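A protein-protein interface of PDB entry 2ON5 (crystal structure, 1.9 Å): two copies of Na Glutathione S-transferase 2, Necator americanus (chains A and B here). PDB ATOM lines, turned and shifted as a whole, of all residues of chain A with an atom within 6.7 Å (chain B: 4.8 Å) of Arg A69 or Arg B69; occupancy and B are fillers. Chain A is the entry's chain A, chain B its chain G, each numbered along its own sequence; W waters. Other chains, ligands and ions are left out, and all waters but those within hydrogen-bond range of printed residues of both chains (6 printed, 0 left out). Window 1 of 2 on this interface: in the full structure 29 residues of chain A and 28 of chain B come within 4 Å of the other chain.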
ATOM      1  N   ILE A  18       8.003  22.931  27.569  1.00  0.00           N
ATOM      2  CA  ILE A  18       7.226  24.140  27.224  1.00  0.00           C
ATOM      3  C   ILE A  18       8.205  25.307  27.053  1.00  0.00           C
ATOM      4  O   ILE A  18       8.131  26.087  26.083  1.00  0.00           O
ATOM      5  CB  ILE A  18       6.183  24.464  28.314  1.00  0.00           C
ATOM      6  CG1 ILE A  18       5.060  23.413  28.343  1.00  0.00           C
ATOM      7  CG2 ILE A  18       5.603  25.873  28.136  1.00  0.00           C
ATOM      8  CD1 ILE A  18       4.447  23.230  29.760  1.00  0.00           C
ATOM      9  N   ILE A  21       9.761  24.834  23.711  1.00  0.00           N
ATOM     10  CA  ILE A  21       8.873  25.277  22.616  1.00  0.00           C
ATOM     11  C   ILE A  21       9.024  26.792  22.406  1.00  0.00           C
ATOM     12  O   ILE A  21       9.180  27.263  21.262  1.00  0.00           O
ATOM     13  CB  ILE A  21       7.419  24.925  22.885  1.00  0.00           C
ATOM     14  CG1 ILE A  21       7.237  23.391  22.818  1.00  0.00           C
ATOM     15  CG2 ILE A  21       6.500  25.723  21.905  1.00  0.00           C
ATOM     16  CD1 ILE A  21       5.880  22.871  23.431  1.00  0.00           C
ATOM     17  N   SER A  64       0.406  20.328  31.823  1.00  0.00           N
ATOM     18  CA  SER A  64       1.628  20.474  31.019  1.00  0.00           C
ATOM     19  C   SER A  64       1.470  20.041  29.549  1.00  0.00           C
ATOM     20  O   SER A  64       1.935  20.754  28.659  1.00  0.00           O
ATOM     21  CB  SER A  64       2.821  19.755  31.671  1.00  0.00           C
ATOM     22  OG  SER A  64       2.590  18.340  31.694  1.00  0.00           O
ATOM     23  N   PHE A  65       0.811  18.908  29.288  1.00  0.00           N
ATOM     24  CA  PHE A  65       0.582  18.460  27.893  1.00  0.00           C
ATOM     25  C   PHE A  65      -0.419  19.318  27.144  1.00  0.00           C
ATOM     26  O   PHE A  65      -0.255  19.535  25.943  1.00  0.00           O
ATOM     27  CB  PHE A  65       0.198  16.982  27.814  1.00  0.00           C
ATOM     28  CG  PHE A  65       1.310  16.043  28.278  1.00  0.00           C
ATOM     29  CD1 PHE A  65       1.498  15.770  29.639  1.00  0.00           C
ATOM     30  CD2 PHE A  65       2.194  15.487  27.364  1.00  0.00           C
ATOM     31  CE1 PHE A  65       2.553  14.905  30.081  1.00  0.00           C
ATOM     32  CE2 PHE A  65       3.226  14.613  27.778  1.00  0.00           C
ATOM     33  CZ  PHE A  65       3.408  14.318  29.132  1.00  0.00           C
ATOM     34  N   ALA A  66      -1.466  19.795  27.832  1.00  0.00           N
ATOM     35  CA  ALA A  66      -2.408  20.714  27.177  1.00  0.00           C
ATOM     36  C   ALA A  66      -1.665  21.994  26.773  1.00  0.00           C
ATOM     37  O   ALA A  66      -1.849  22.530  25.670  1.00  0.00           O
ATOM     38  CB  ALA A  66      -3.584  21.024  28.072  1.00  0.00           C
ATOM     39  N   ILE A  67      -0.807  22.472  27.665  1.00  0.00           N
ATOM     40  CA  ILE A  67       0.007  23.653  27.375  1.00  0.00           C
ATOM     41  C   ILE A  67       0.991  23.379  26.237  1.00  0.00           C
ATOM     42  O   ILE A  67       1.122  24.198  25.329  1.00  0.00           O
ATOM     43  CB  ILE A  67       0.799  24.116  28.637  1.00  0.00           C
ATOM     44  CG1 ILE A  67      -0.192  24.593  29.710  1.00  0.00           C
ATOM     45  CG2 ILE A  67       1.784  25.272  28.240  1.00  0.00           C
ATOM     46  CD1 ILE A  67       0.420  24.621  31.165  1.00  0.00           C
ATOM     47  N   ALA A  68       1.712  22.255  26.302  1.00  0.00           N
ATOM     48  CA  ALA A  68       2.689  21.946  25.263  1.00  0.00           C
ATOM     49  C   ALA A  68       2.025  21.874  23.889  1.00  0.00           C
ATOM     50  O   ALA A  68       2.554  22.417  22.913  1.00  0.00           O
ATOM     51  CB  ALA A  68       3.438  20.615  25.561  1.00  0.00           C
ATOM     52  N   ARG A  69       0.878  21.201  23.817  1.00  0.00           N
ATOM     53  CA  ARG A  69       0.185  20.988  22.517  1.00  0.00           C
ATOM     54  C   ARG A  69      -0.334  22.331  21.969  1.00  0.00           C
ATOM     55  O   ARG A  69      -0.189  22.623  20.785  1.00  0.00           O
ATOM     56  CB  ARG A  69      -0.999  20.033  22.664  1.00  0.00           C
ATOM     57  CG  ARG A  69      -1.748  19.692  21.325  1.00  0.00           C
ATOM     58  CD  ARG A  69      -2.874  18.640  21.537  1.00  0.00           C
ATOM     59  NE  ARG A  69      -2.299  17.470  22.183  1.00  0.00           N
ATOM     60  CZ  ARG A  69      -2.418  17.154  23.471  1.00  0.00           C
ATOM     61  NH1 ARG A  69      -3.174  17.871  24.292  1.00  0.00           N
ATOM     62  NH2 ARG A  69      -1.772  16.099  23.937  1.00  0.00           N
ATOM     63  N   TYR A  70      -0.956  23.112  22.846  1.00  0.00           N
ATOM     64  CA  TYR A  70      -1.474  24.445  22.470  1.00  0.00           C
ATOM     65  C   TYR A  70      -0.400  25.343  21.801  1.00  0.00           C
ATOM     66  O   TYR A  70      -0.608  25.897  20.711  1.00  0.00           O
ATOM     67  CB  TYR A  70      -2.060  25.142  23.703  1.00  0.00           C
ATOM     68  CG  TYR A  70      -2.508  26.572  23.398  1.00  0.00           C
ATOM     69  CD1 TYR A  70      -3.594  26.799  22.547  1.00  0.00           C
ATOM     70  CD2 TYR A  70      -1.809  27.673  23.908  1.00  0.00           C
ATOM     71  CE1 TYR A  70      -4.005  28.080  22.230  1.00  0.00           C
ATOM     72  CE2 TYR A  70      -2.221  28.997  23.611  1.00  0.00           C
ATOM     73  CZ  TYR A  70      -3.306  29.181  22.751  1.00  0.00           C
ATOM     74  OH  TYR A  70      -3.733  30.453  22.417  1.00  0.00           O
ATOM     75  N   LEU A  71       0.742  25.496  22.471  1.00  0.00           N
ATOM     76  CA  LEU A  71       1.881  26.235  21.904  1.00  0.00           C
ATOM     77  C   LEU A  71       2.515  25.553  20.692  1.00  0.00           C
ATOM     78  O   LEU A  71       2.915  26.229  19.728  1.00  0.00           O
ATOM     79  CB  LEU A  71       2.944  26.529  22.975  1.00  0.00           C
ATOM     80  CG  LEU A  71       2.447  27.278  24.206  1.00  0.00           C
ATOM     81  CD1 LEU A  71       3.438  27.167  25.356  1.00  0.00           C
ATOM     82  CD2 LEU A  71       2.031  28.752  23.901  1.00  0.00           C
ATOM     83  N   SER A  72       2.573  24.223  20.697  1.00  0.00           N
ATOM     84  CA  SER A  72       3.148  23.525  19.557  1.00  0.00           C
ATOM     85  C   SER A  72       2.261  23.709  18.322  1.00  0.00           C
ATOM     86  O   SER A  72       2.761  23.907  17.228  1.00  0.00           O
ATOM     87  CB  SER A  72       3.326  22.047  19.851  1.00  0.00           C
ATOM     88  OG  SER A  72       4.336  21.904  20.825  1.00  0.00           O
ATOM     89  N   ARG A  73       0.947  23.646  18.499  1.00  0.00           N
ATOM     90  CA  ARG A  73       0.056  23.932  17.363  1.00  0.00           C
ATOM     91  C   ARG A  73       0.250  25.344  16.838  1.00  0.00           C
ATOM     92  O   ARG A  73       0.188  25.582  15.631  1.00  0.00           O
ATOM     93  CB  ARG A  73      -1.398  23.701  17.732  1.00  0.00           C
ATOM     94  CG  ARG A  73      -1.751  22.210  17.756  1.00  0.00           C
ATOM     95  CD  ARG A  73      -3.250  21.886  17.728  1.00  0.00           C
ATOM     96  NE  ARG A  73      -4.123  23.027  17.497  1.00  0.00           N
ATOM     97  CZ  ARG A  73      -5.462  22.992  17.628  1.00  0.00           C
ATOM     98  NH1 ARG A  73      -6.076  21.873  17.998  1.00  0.00           N
ATOM     99  NH2 ARG A  73      -6.180  24.098  17.445  1.00  0.00           N
ATOM    100  N   LYS A  74       0.450  26.293  17.738  1.00  0.00           N
ATOM    101  CA  LYS A  74       0.608  27.704  17.334  1.00  0.00           C
ATOM    102  C   LYS A  74       1.940  27.942  16.590  1.00  0.00           C
ATOM    103  O   LYS A  74       2.031  28.771  15.649  1.00  0.00           O
ATOM    104  CB  LYS A  74       0.505  28.597  18.591  1.00  0.00           C
ATOM    105  CG  LYS A  74       0.538  30.083  18.326  1.00  0.00           C
ATOM    106  CD  LYS A  74       0.646  30.851  19.616  1.00  0.00           C
ATOM    107  CE  LYS A  74      -0.601  30.653  20.471  1.00  0.00           C
ATOM    108  NZ  LYS A  74      -1.712  31.478  19.974  1.00  0.00           N
ATOM    109  N   PHE A  77       5.213  22.865  15.960  1.00  0.00           N
ATOM    110  CA  PHE A  77       5.870  21.678  16.552  1.00  0.00           C
ATOM    111  C   PHE A  77       4.905  20.565  16.990  1.00  0.00           C
ATOM    112  O   PHE A  77       5.233  19.759  17.850  1.00  0.00           O
ATOM    113  CB  PHE A  77       6.727  22.105  17.740  1.00  0.00           C
ATOM    114  CG  PHE A  77       7.644  23.235  17.405  1.00  0.00           C
ATOM    115  CD1 PHE A  77       8.673  23.050  16.478  1.00  0.00           C
ATOM    116  CD2 PHE A  77       7.440  24.478  17.940  1.00  0.00           C
ATOM    117  CE1 PHE A  77       9.508  24.112  16.117  1.00  0.00           C
ATOM    118  CE2 PHE A  77       8.267  25.550  17.589  1.00  0.00           C
ATOM    119  CZ  PHE A  77       9.291  25.358  16.678  1.00  0.00           C
ATOM    120  N   ALA A  78       3.704  20.560  16.424  1.00  0.00           N
ATOM    121  CA  ALA A  78       2.669  19.601  16.846  1.00  0.00           C
ATOM    122  C   ALA A  78       2.555  18.398  15.896  1.00  0.00           C
ATOM    123  O   ALA A  78       1.823  17.447  16.186  1.00  0.00           O
ATOM    124  CB  ALA A  78       1.285  20.293  16.930  1.00  0.00           C
ATOM    125  N   GLU A  85      -0.345  14.784  13.822  1.00  0.00           N
ATOM    126  CA  GLU A  85      -0.596  15.416  15.140  1.00  0.00           C
ATOM    127  C   GLU A  85      -1.123  14.398  16.147  1.00  0.00           C
ATOM    128  O   GLU A  85      -0.753  14.423  17.327  1.00  0.00           O
ATOM    129  CB  GLU A  85      -1.582  16.566  15.012  1.00  0.00           C
ATOM    130  CG  GLU A  85      -1.043  17.778  14.299  1.00  0.00           C
ATOM    131  CD  GLU A  85      -2.074  18.878  14.247  1.00  0.00           C
ATOM    132  OE1 GLU A  85      -2.229  19.595  15.248  1.00  0.00           O
ATOM    133  OE2 GLU A  85      -2.775  18.968  13.227  1.00  0.00           O
ATOM    134  N   ALA A  86      -1.973  13.491  15.667  1.00  0.00           N
ATOM    135  CA  ALA A  86      -2.536  12.448  16.523  1.00  0.00           C
ATOM    136  C   ALA A  86      -1.438  11.478  16.917  1.00  0.00           C
ATOM    137  O   ALA A  86      -1.376  11.079  18.080  1.00  0.00           O
ATOM    138  CB  ALA A  86      -3.673  11.730  15.830  1.00  0.00           C
ATOM    139  N   VAL A  88       1.732  12.096  17.108  1.00  0.00           N
ATOM    140  CA  VAL A  88       2.542  12.841  18.117  1.00  0.00           C
ATOM    141  C   VAL A  88       1.916  12.761  19.523  1.00  0.00           C
ATOM    142  O   VAL A  88       2.616  12.444  20.511  1.00  0.00           O
ATOM    143  CB  VAL A  88       2.775  14.308  17.685  1.00  0.00           C
ATOM    144  CG1 VAL A  88       3.464  15.156  18.847  1.00  0.00           C
ATOM    145  CG2 VAL A  88       3.628  14.347  16.411  1.00  0.00           C
ATOM    146  N   ASP A  89       0.612  13.042  19.609  1.00  0.00           N
ATOM    147  CA  ASP A  89      -0.159  12.875  20.845  1.00  0.00           C
ATOM    148  C   ASP A  89      -0.016  11.486  21.458  1.00  0.00           C
ATOM    149  O   ASP A  89       0.167  11.363  22.675  1.00  0.00           O
ATOM    150  CB  ASP A  89      -1.656  13.167  20.625  1.00  0.00           C
ATOM    151  CG  ASP A  89      -1.945  14.632  20.318  1.00  0.00           C
ATOM    152  OD1 ASP A  89      -0.995  15.439  20.339  1.00  0.00           O
ATOM    153  OD2 ASP A  89      -3.148  14.960  20.121  1.00  0.00           O
ATOM    154  N   SER A  90      -0.144  10.446  20.638  1.00  0.00           N
ATOM    155  CA  SER A  90      -0.064   9.053  21.161  1.00  0.00           C
ATOM    156  C   SER A  90       1.310   8.739  21.785  1.00  0.00           C
ATOM    157  O   SER A  90       1.382   8.079  22.837  1.00  0.00           O
ATOM    158  CB  SER A  90      -0.422   8.036  20.055  1.00  0.00           C
ATOM    159  OG  SER A  90       0.621   7.871  19.115  1.00  0.00           O
ATOM    160  N   ALA A  92       3.335  11.109  23.040  1.00  0.00           N
ATOM    161  CA  ALA A  92       3.397  11.926  24.248  1.00  0.00           C
ATOM    162  C   ALA A  92       2.634  11.253  25.376  1.00  0.00           C
ATOM    163  O   ALA A  92       3.060  11.297  26.527  1.00  0.00           O
ATOM    164  CB  ALA A  92       2.828  13.354  23.979  1.00  0.00           C
ATOM    165  N   ASP A  93       1.499  10.642  25.039  1.00  0.00           N
ATOM    166  CA  ASP A  93       0.705   9.914  26.024  1.00  0.00           C
ATOM    167  C   ASP A  93       1.434   8.679  26.536  1.00  0.00           C
ATOM    168  O   ASP A  93       1.360   8.372  27.734  1.00  0.00           O
ATOM    169  CB  ASP A  93      -0.663   9.520  25.461  1.00  0.00           C
ATOM    170  CG  ASP A  93      -1.711  10.611  25.642  1.00  0.00           C
ATOM    171  OD1 ASP A  93      -1.402  11.660  26.252  1.00  0.00           O
ATOM    172  OD2 ASP A  93      -2.854  10.408  25.173  1.00  0.00           O
ATOM    173  N   TYR A 155       6.849  18.324  19.886  1.00  0.00           N
ATOM    174  CA  TYR A 155       6.940  18.375  21.362  1.00  0.00           C
ATOM    175  C   TYR A 155       7.184  16.998  21.987  1.00  0.00           C
ATOM    176  O   TYR A 155       7.714  16.897  23.104  1.00  0.00           O
ATOM    177  CB  TYR A 155       5.753  19.123  21.985  1.00  0.00           C
ATOM    178  CG  TYR A 155       4.455  18.354  22.010  1.00  0.00           C
ATOM    179  CD1 TYR A 155       4.148  17.549  23.101  1.00  0.00           C
ATOM    180  CD2 TYR A 155       3.532  18.430  20.955  1.00  0.00           C
ATOM    181  CE1 TYR A 155       2.963  16.814  23.148  1.00  0.00           C
ATOM    182  CE2 TYR A 155       2.323  17.692  20.999  1.00  0.00           C
ATOM    183  CZ  TYR A 155       2.065  16.885  22.103  1.00  0.00           C
ATOM    184  OH  TYR A 155       0.915  16.139  22.193  1.00  0.00           O
ATOM    185  N   PHE B  65      -6.862   8.910  24.678  1.00  0.00           N
ATOM    186  CA  PHE B  65      -7.105  10.358  24.563  1.00  0.00           C
ATOM    187  C   PHE B  65      -6.624  10.915  23.213  1.00  0.00           C
ATOM    188  O   PHE B  65      -7.231  11.832  22.680  1.00  0.00           O
ATOM    189  CB  PHE B  65      -6.490  11.141  25.740  1.00  0.00           C
ATOM    190  CG  PHE B  65      -7.158  10.870  27.073  1.00  0.00           C
ATOM    191  CD1 PHE B  65      -6.852   9.705  27.801  1.00  0.00           C
ATOM    192  CD2 PHE B  65      -8.053  11.775  27.615  1.00  0.00           C
ATOM    193  CE1 PHE B  65      -7.468   9.448  29.043  1.00  0.00           C
ATOM    194  CE2 PHE B  65      -8.680  11.543  28.854  1.00  0.00           C
ATOM    195  CZ  PHE B  65      -8.386  10.377  29.578  1.00  0.00           C
ATOM    196  N   ALA B  66      -5.525  10.385  22.670  1.00  0.00           N
ATOM    197  CA  ALA B  66      -5.083  10.788  21.337  1.00  0.00           C
ATOM    198  C   ALA B  66      -6.163  10.406  20.315  1.00  0.00           C
ATOM    199  O   ALA B  66      -6.526  11.201  19.433  1.00  0.00           O
ATOM    200  CB  ALA B  66      -3.751  10.100  20.976  1.00  0.00           C
ATOM    201  N   ILE B  67      -6.681   9.191  20.429  1.00  0.00           N
ATOM    202  CA  ILE B  67      -7.794   8.764  19.546  1.00  0.00           C
ATOM    203  C   ILE B  67      -8.998   9.716  19.696  1.00  0.00           C
ATOM    204  O   ILE B  67      -9.548  10.212  18.708  1.00  0.00           O
ATOM    205  CB  ILE B  67      -8.222   7.311  19.843  1.00  0.00           C
ATOM    206  CG1 ILE B  67      -7.034   6.361  19.625  1.00  0.00           C
ATOM    207  CG2 ILE B  67      -9.396   6.897  18.891  1.00  0.00           C
ATOM    208  CD1 ILE B  67      -7.244   4.886  20.135  1.00  0.00           C
ATOM    209  N   ALA B  68      -9.429   9.934  20.927  1.00  0.00           N
ATOM    210  CA  ALA B  68     -10.618  10.776  21.184  1.00  0.00           C
ATOM    211  C   ALA B  68     -10.472  12.192  20.608  1.00  0.00           C
ATOM    212  O   ALA B  68     -11.395  12.704  19.954  1.00  0.00           O
ATOM    213  CB  ALA B  68     -10.904  10.823  22.674  1.00  0.00           C
ATOM    214  N   ARG B  69      -9.308  12.817  20.836  1.00  0.00           N
ATOM    215  CA  ARG B  69      -9.023  14.155  20.308  1.00  0.00           C
ATOM    216  C   ARG B  69      -9.006  14.145  18.782  1.00  0.00           C
ATOM    217  O   ARG B  69      -9.581  15.021  18.163  1.00  0.00           O
ATOM    218  CB  ARG B  69      -7.710  14.732  20.862  1.00  0.00           C
ATOM    219  CG  ARG B  69      -7.463  16.229  20.517  1.00  0.00           C
ATOM    220  CD  ARG B  69      -6.127  16.719  21.084  1.00  0.00           C
ATOM    221  NE  ARG B  69      -6.138  16.510  22.513  1.00  0.00           N
ATOM    222  CZ  ARG B  69      -5.521  15.511  23.142  1.00  0.00           C
ATOM    223  NH1 ARG B  69      -4.716  14.668  22.499  1.00  0.00           N
ATOM    224  NH2 ARG B  69      -5.692  15.382  24.440  1.00  0.00           N
ATOM    225  N   TYR B  70      -8.353  13.156  18.176  1.00  0.00           N
ATOM    226  CA  TYR B  70      -8.262  13.102  16.729  1.00  0.00           C
ATOM    227  C   TYR B  70      -9.673  13.068  16.100  1.00  0.00           C
ATOM    228  O   TYR B  70      -9.974  13.844  15.198  1.00  0.00           O
ATOM    229  CB  TYR B  70      -7.429  11.880  16.289  1.00  0.00           C
ATOM    230  CG  TYR B  70      -7.447  11.664  14.792  1.00  0.00           C
ATOM    231  CD1 TYR B  70      -6.753  12.522  13.944  1.00  0.00           C
ATOM    232  CD2 TYR B  70      -8.174  10.605  14.217  1.00  0.00           C
ATOM    233  CE1 TYR B  70      -6.763  12.344  12.551  1.00  0.00           C
ATOM    234  CE2 TYR B  70      -8.179  10.411  12.825  1.00  0.00           C
ATOM    235  CZ  TYR B  70      -7.476  11.290  12.011  1.00  0.00           C
ATOM    236  OH  TYR B  70      -7.485  11.147  10.633  1.00  0.00           O
ATOM    237  N   LEU B  71     -10.519  12.165  16.589  1.00  0.00           N
ATOM    238  CA  LEU B  71     -11.914  12.051  16.118  1.00  0.00           C
ATOM    239  C   LEU B  71     -12.763  13.271  16.489  1.00  0.00           C
ATOM    240  O   LEU B  71     -13.585  13.733  15.688  1.00  0.00           O
ATOM    241  CB  LEU B  71     -12.564  10.775  16.669  1.00  0.00           C
ATOM    242  CG  LEU B  71     -11.892   9.468  16.234  1.00  0.00           C
ATOM    243  CD1 LEU B  71     -12.515   8.342  16.983  1.00  0.00           C
ATOM    244  CD2 LEU B  71     -12.020   9.270  14.731  1.00  0.00           C
ATOM    245  N   SER B  72     -12.566  13.799  17.697  1.00  0.00           N
ATOM    246  CA  SER B  72     -13.278  15.007  18.119  1.00  0.00           C
ATOM    247  C   SER B  72     -12.977  16.223  17.224  1.00  0.00           C
ATOM    248  O   SER B  72     -13.913  16.980  16.862  1.00  0.00           O
ATOM    249  CB  SER B  72     -13.024  15.322  19.608  1.00  0.00           C
ATOM    250  OG  SER B  72     -13.542  14.313  20.443  1.00  0.00           O
ATOM    251  N   ARG B  73     -11.700  16.428  16.866  1.00  0.00           N
ATOM    252  CA  ARG B  73     -11.356  17.513  15.921  1.00  0.00           C
ATOM    253  C   ARG B  73     -12.004  17.333  14.575  1.00  0.00           C
ATOM    254  O   ARG B  73     -12.430  18.302  13.962  1.00  0.00           O
ATOM    255  CB  ARG B  73      -9.842  17.695  15.705  1.00  0.00           C
ATOM    256  CG  ARG B  73      -9.135  18.379  16.859  1.00  0.00           C
ATOM    257  CD  ARG B  73      -7.595  18.538  16.647  1.00  0.00           C
ATOM    258  NE  ARG B  73      -7.231  18.538  15.237  1.00  0.00           N
ATOM    259  CZ  ARG B  73      -5.989  18.697  14.770  1.00  0.00           C
ATOM    260  NH1 ARG B  73      -4.969  18.924  15.608  1.00  0.00           N
ATOM    261  NH2 ARG B  73      -5.775  18.626  13.457  1.00  0.00           N
ATOM    262  N   ALA B  78     -14.218  18.942  19.801  1.00  0.00           N
ATOM    263  CA  ALA B  78     -12.911  19.233  20.432  1.00  0.00           C
ATOM    264  C   ALA B  78     -12.843  20.595  21.101  1.00  0.00           C
ATOM    265  O   ALA B  78     -11.897  20.878  21.837  1.00  0.00           O
ATOM    266  CB  ALA B  78     -11.748  19.092  19.398  1.00  0.00           C
ATOM    267  N   ASP B  89      -8.706  20.024  26.436  1.00  0.00           N
ATOM    268  CA  ASP B  89      -7.573  19.124  26.750  1.00  0.00           C
ATOM    269  C   ASP B  89      -7.210  19.147  28.234  1.00  0.00           C
ATOM    270  O   ASP B  89      -6.898  18.104  28.825  1.00  0.00           O
ATOM    271  CB  ASP B  89      -6.306  19.504  25.956  1.00  0.00           C
ATOM    272  CG  ASP B  89      -6.419  19.203  24.460  1.00  0.00           C
ATOM    273  OD1 ASP B  89      -5.458  19.572  23.771  1.00  0.00           O
ATOM    274  OD2 ASP B  89      -7.441  18.602  23.965  1.00  0.00           O
ATOM    275  N   TYR B 155     -15.520  16.007  24.010  1.00  0.00           N
ATOM    276  CA  TYR B 155     -15.063  14.696  24.461  1.00  0.00           C
ATOM    277  C   TYR B 155     -14.758  14.730  25.946  1.00  0.00           C
ATOM    278  O   TYR B 155     -14.868  13.698  26.613  1.00  0.00           O
ATOM    279  CB  TYR B 155     -13.891  14.167  23.624  1.00  0.00           C
ATOM    280  CG  TYR B 155     -12.519  14.768  23.940  1.00  0.00           C
ATOM    281  CD1 TYR B 155     -11.667  14.168  24.889  1.00  0.00           C
ATOM    282  CD2 TYR B 155     -12.063  15.915  23.266  1.00  0.00           C
ATOM    283  CE1 TYR B 155     -10.388  14.719  25.190  1.00  0.00           C
ATOM    284  CE2 TYR B 155     -10.792  16.482  23.557  1.00  0.00           C
ATOM    285  CZ  TYR B 155      -9.971  15.874  24.515  1.00  0.00           C
ATOM    286  OH  TYR B 155      -8.739  16.413  24.783  1.00  0.00           O
HETATM  287  O   HOH W   1      -3.342  12.722  24.138  1.00  0.00           O
HETATM  288  O   HOH W   2      -5.910  20.383  21.155  1.00  0.00           O
HETATM  289  O   HOH W   3      -3.780  21.790  23.817  1.00  0.00           O
HETATM  290  O   HOH W   4      -4.164   8.536  26.016  1.00  0.00           O
HETATM  291  O   HOH W   5      -4.775  21.146  13.770  1.00  0.00           O
HETATM  292  O   HOH W   6      -4.921  13.484  18.643  1.00  0.00           O
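NH1 of Arg A69 is in salt-bridge range of OD1 of Asp B89 (2.9 Å). OE1 of Glu A85 lies within salt-bridge range of NH1 of Arg B73 (2.8 Å). OD2 of Asp A89 lies within salt-bridge range of NH1 of Arg B69 (2.9 Å).
Water W4 lies within hydrogen-bond range of the side-chain carboxylate of Asp A93 (2.4 Å) and the backbone NH of Phe B65 (3.0 Å). Water W1 lies within hydrogen-bond range of OD2 of Asp A93 and NH1 of Arg B69. Water W5 bridges the guanidinium group of Arg B73 (2.7 Å) and the side-chain carboxylate of Glu A85 (3.0 Å). Water W6 lies within hydrogen-bond range of OD2 of Asp A89 (2.7 Å), O of Ala B66 (2.9 Å) and N of Tyr B70 (3.5 Å). Water W2 lies within hydrogen-bond range of OD1 of Asp B89 (2.8 Å) and NH1 of Arg A73 (3.5 Å). Water W3 lies within hydrogen-bond range of O of Ala A66, OD1 of Asp B89 and N of Tyr A70.
The guanidinium group of Arg B69 sits at hydrogen-bond distance from the side-chain hydroxyl of Tyr B155 (3.2 Å). NH2 of Arg A69 is in hydrogen-bond range of OH of Tyr A155, 3.2 Å away. The side-chain carboxylate (OD2) of Asp B89 lies within hydrogen-bond range of the side-chain hydroxyl (OH) of Tyr B155. OD1 of Asp A89 is in salt-bridge range of NE of Arg A69. The side-chain carboxylate (OD1) of Asp A89 sits at hydrogen-bond distance from the side-chain hydroxyl (OH) of Tyr A155 (2.8 Å). The guanidinium group (NE) of Arg B69 lies within salt-bridge range of the side-chain carboxylate (OD2) of Asp B89, 2.9 Å away.
Among the printed residues, merely in contact across the chains: Arg A69 with Arg B69, Ser A90 with Ala B66, Asp A93 with Ala B66, Ala A86 with Tyr B70, Asp A89 with Ala B66, Asp A93 with Phe B65, Ala A66 with Asp B89, Ala A86 with Ala B66 and Arg A73 with Arg B73.
Printed residues of chain B that touch a printed residue of chain A: Phe B65, Ala B66, Arg B69, Tyr B70, Arg B73 and Asp B89. Hydrophobic or aromatic side chains of chain B within 4 Å of the printed part of chain A: Phe B65, Ala B66 and Tyr B70. Of the 23 printed residues of chain A, 8 touch a printed residue of chain B. Hydrophobic or aromatic side chains of chain A that line the printed part of chain B: Ala A66 and Ala A86. Among the printed residues, 12 pairs touch across the chains.
Ala A66 touches Asp B89, and with the chains exchanged Asp A89 touches Ala B66. Arg A69 touches its own counterpart, Arg B69. Arg A69 touches Asp B89, and with the chains exchanged Asp A89 touches Arg B69. Arg A73 touches its own counterpart, Arg B73. Positions printed for both chains: 65, 66, 67, 68, 69, 70, 71, 72, 73, 78, 89 and 155. Of the 12 pairs that touch across the chains among the printed residues, 6 have their exchanged pair printed and touching as well.
Of chain B, only Arg B69 (3.5 Å) and Asp B89 (2.9 Å) come within 4 Å of Arg A69. Arg B69 touches two residues of chain A. Of the printed residues of chain A, Ala B66 touches Ala A86, Asp A89, Ser A90 and Asp A93. Of the printed residues of chain A, Phe B65 touches Asp A93. The nearest residue of chain A that does not touch Arg B69 is Asp A93 (5.4 Å).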
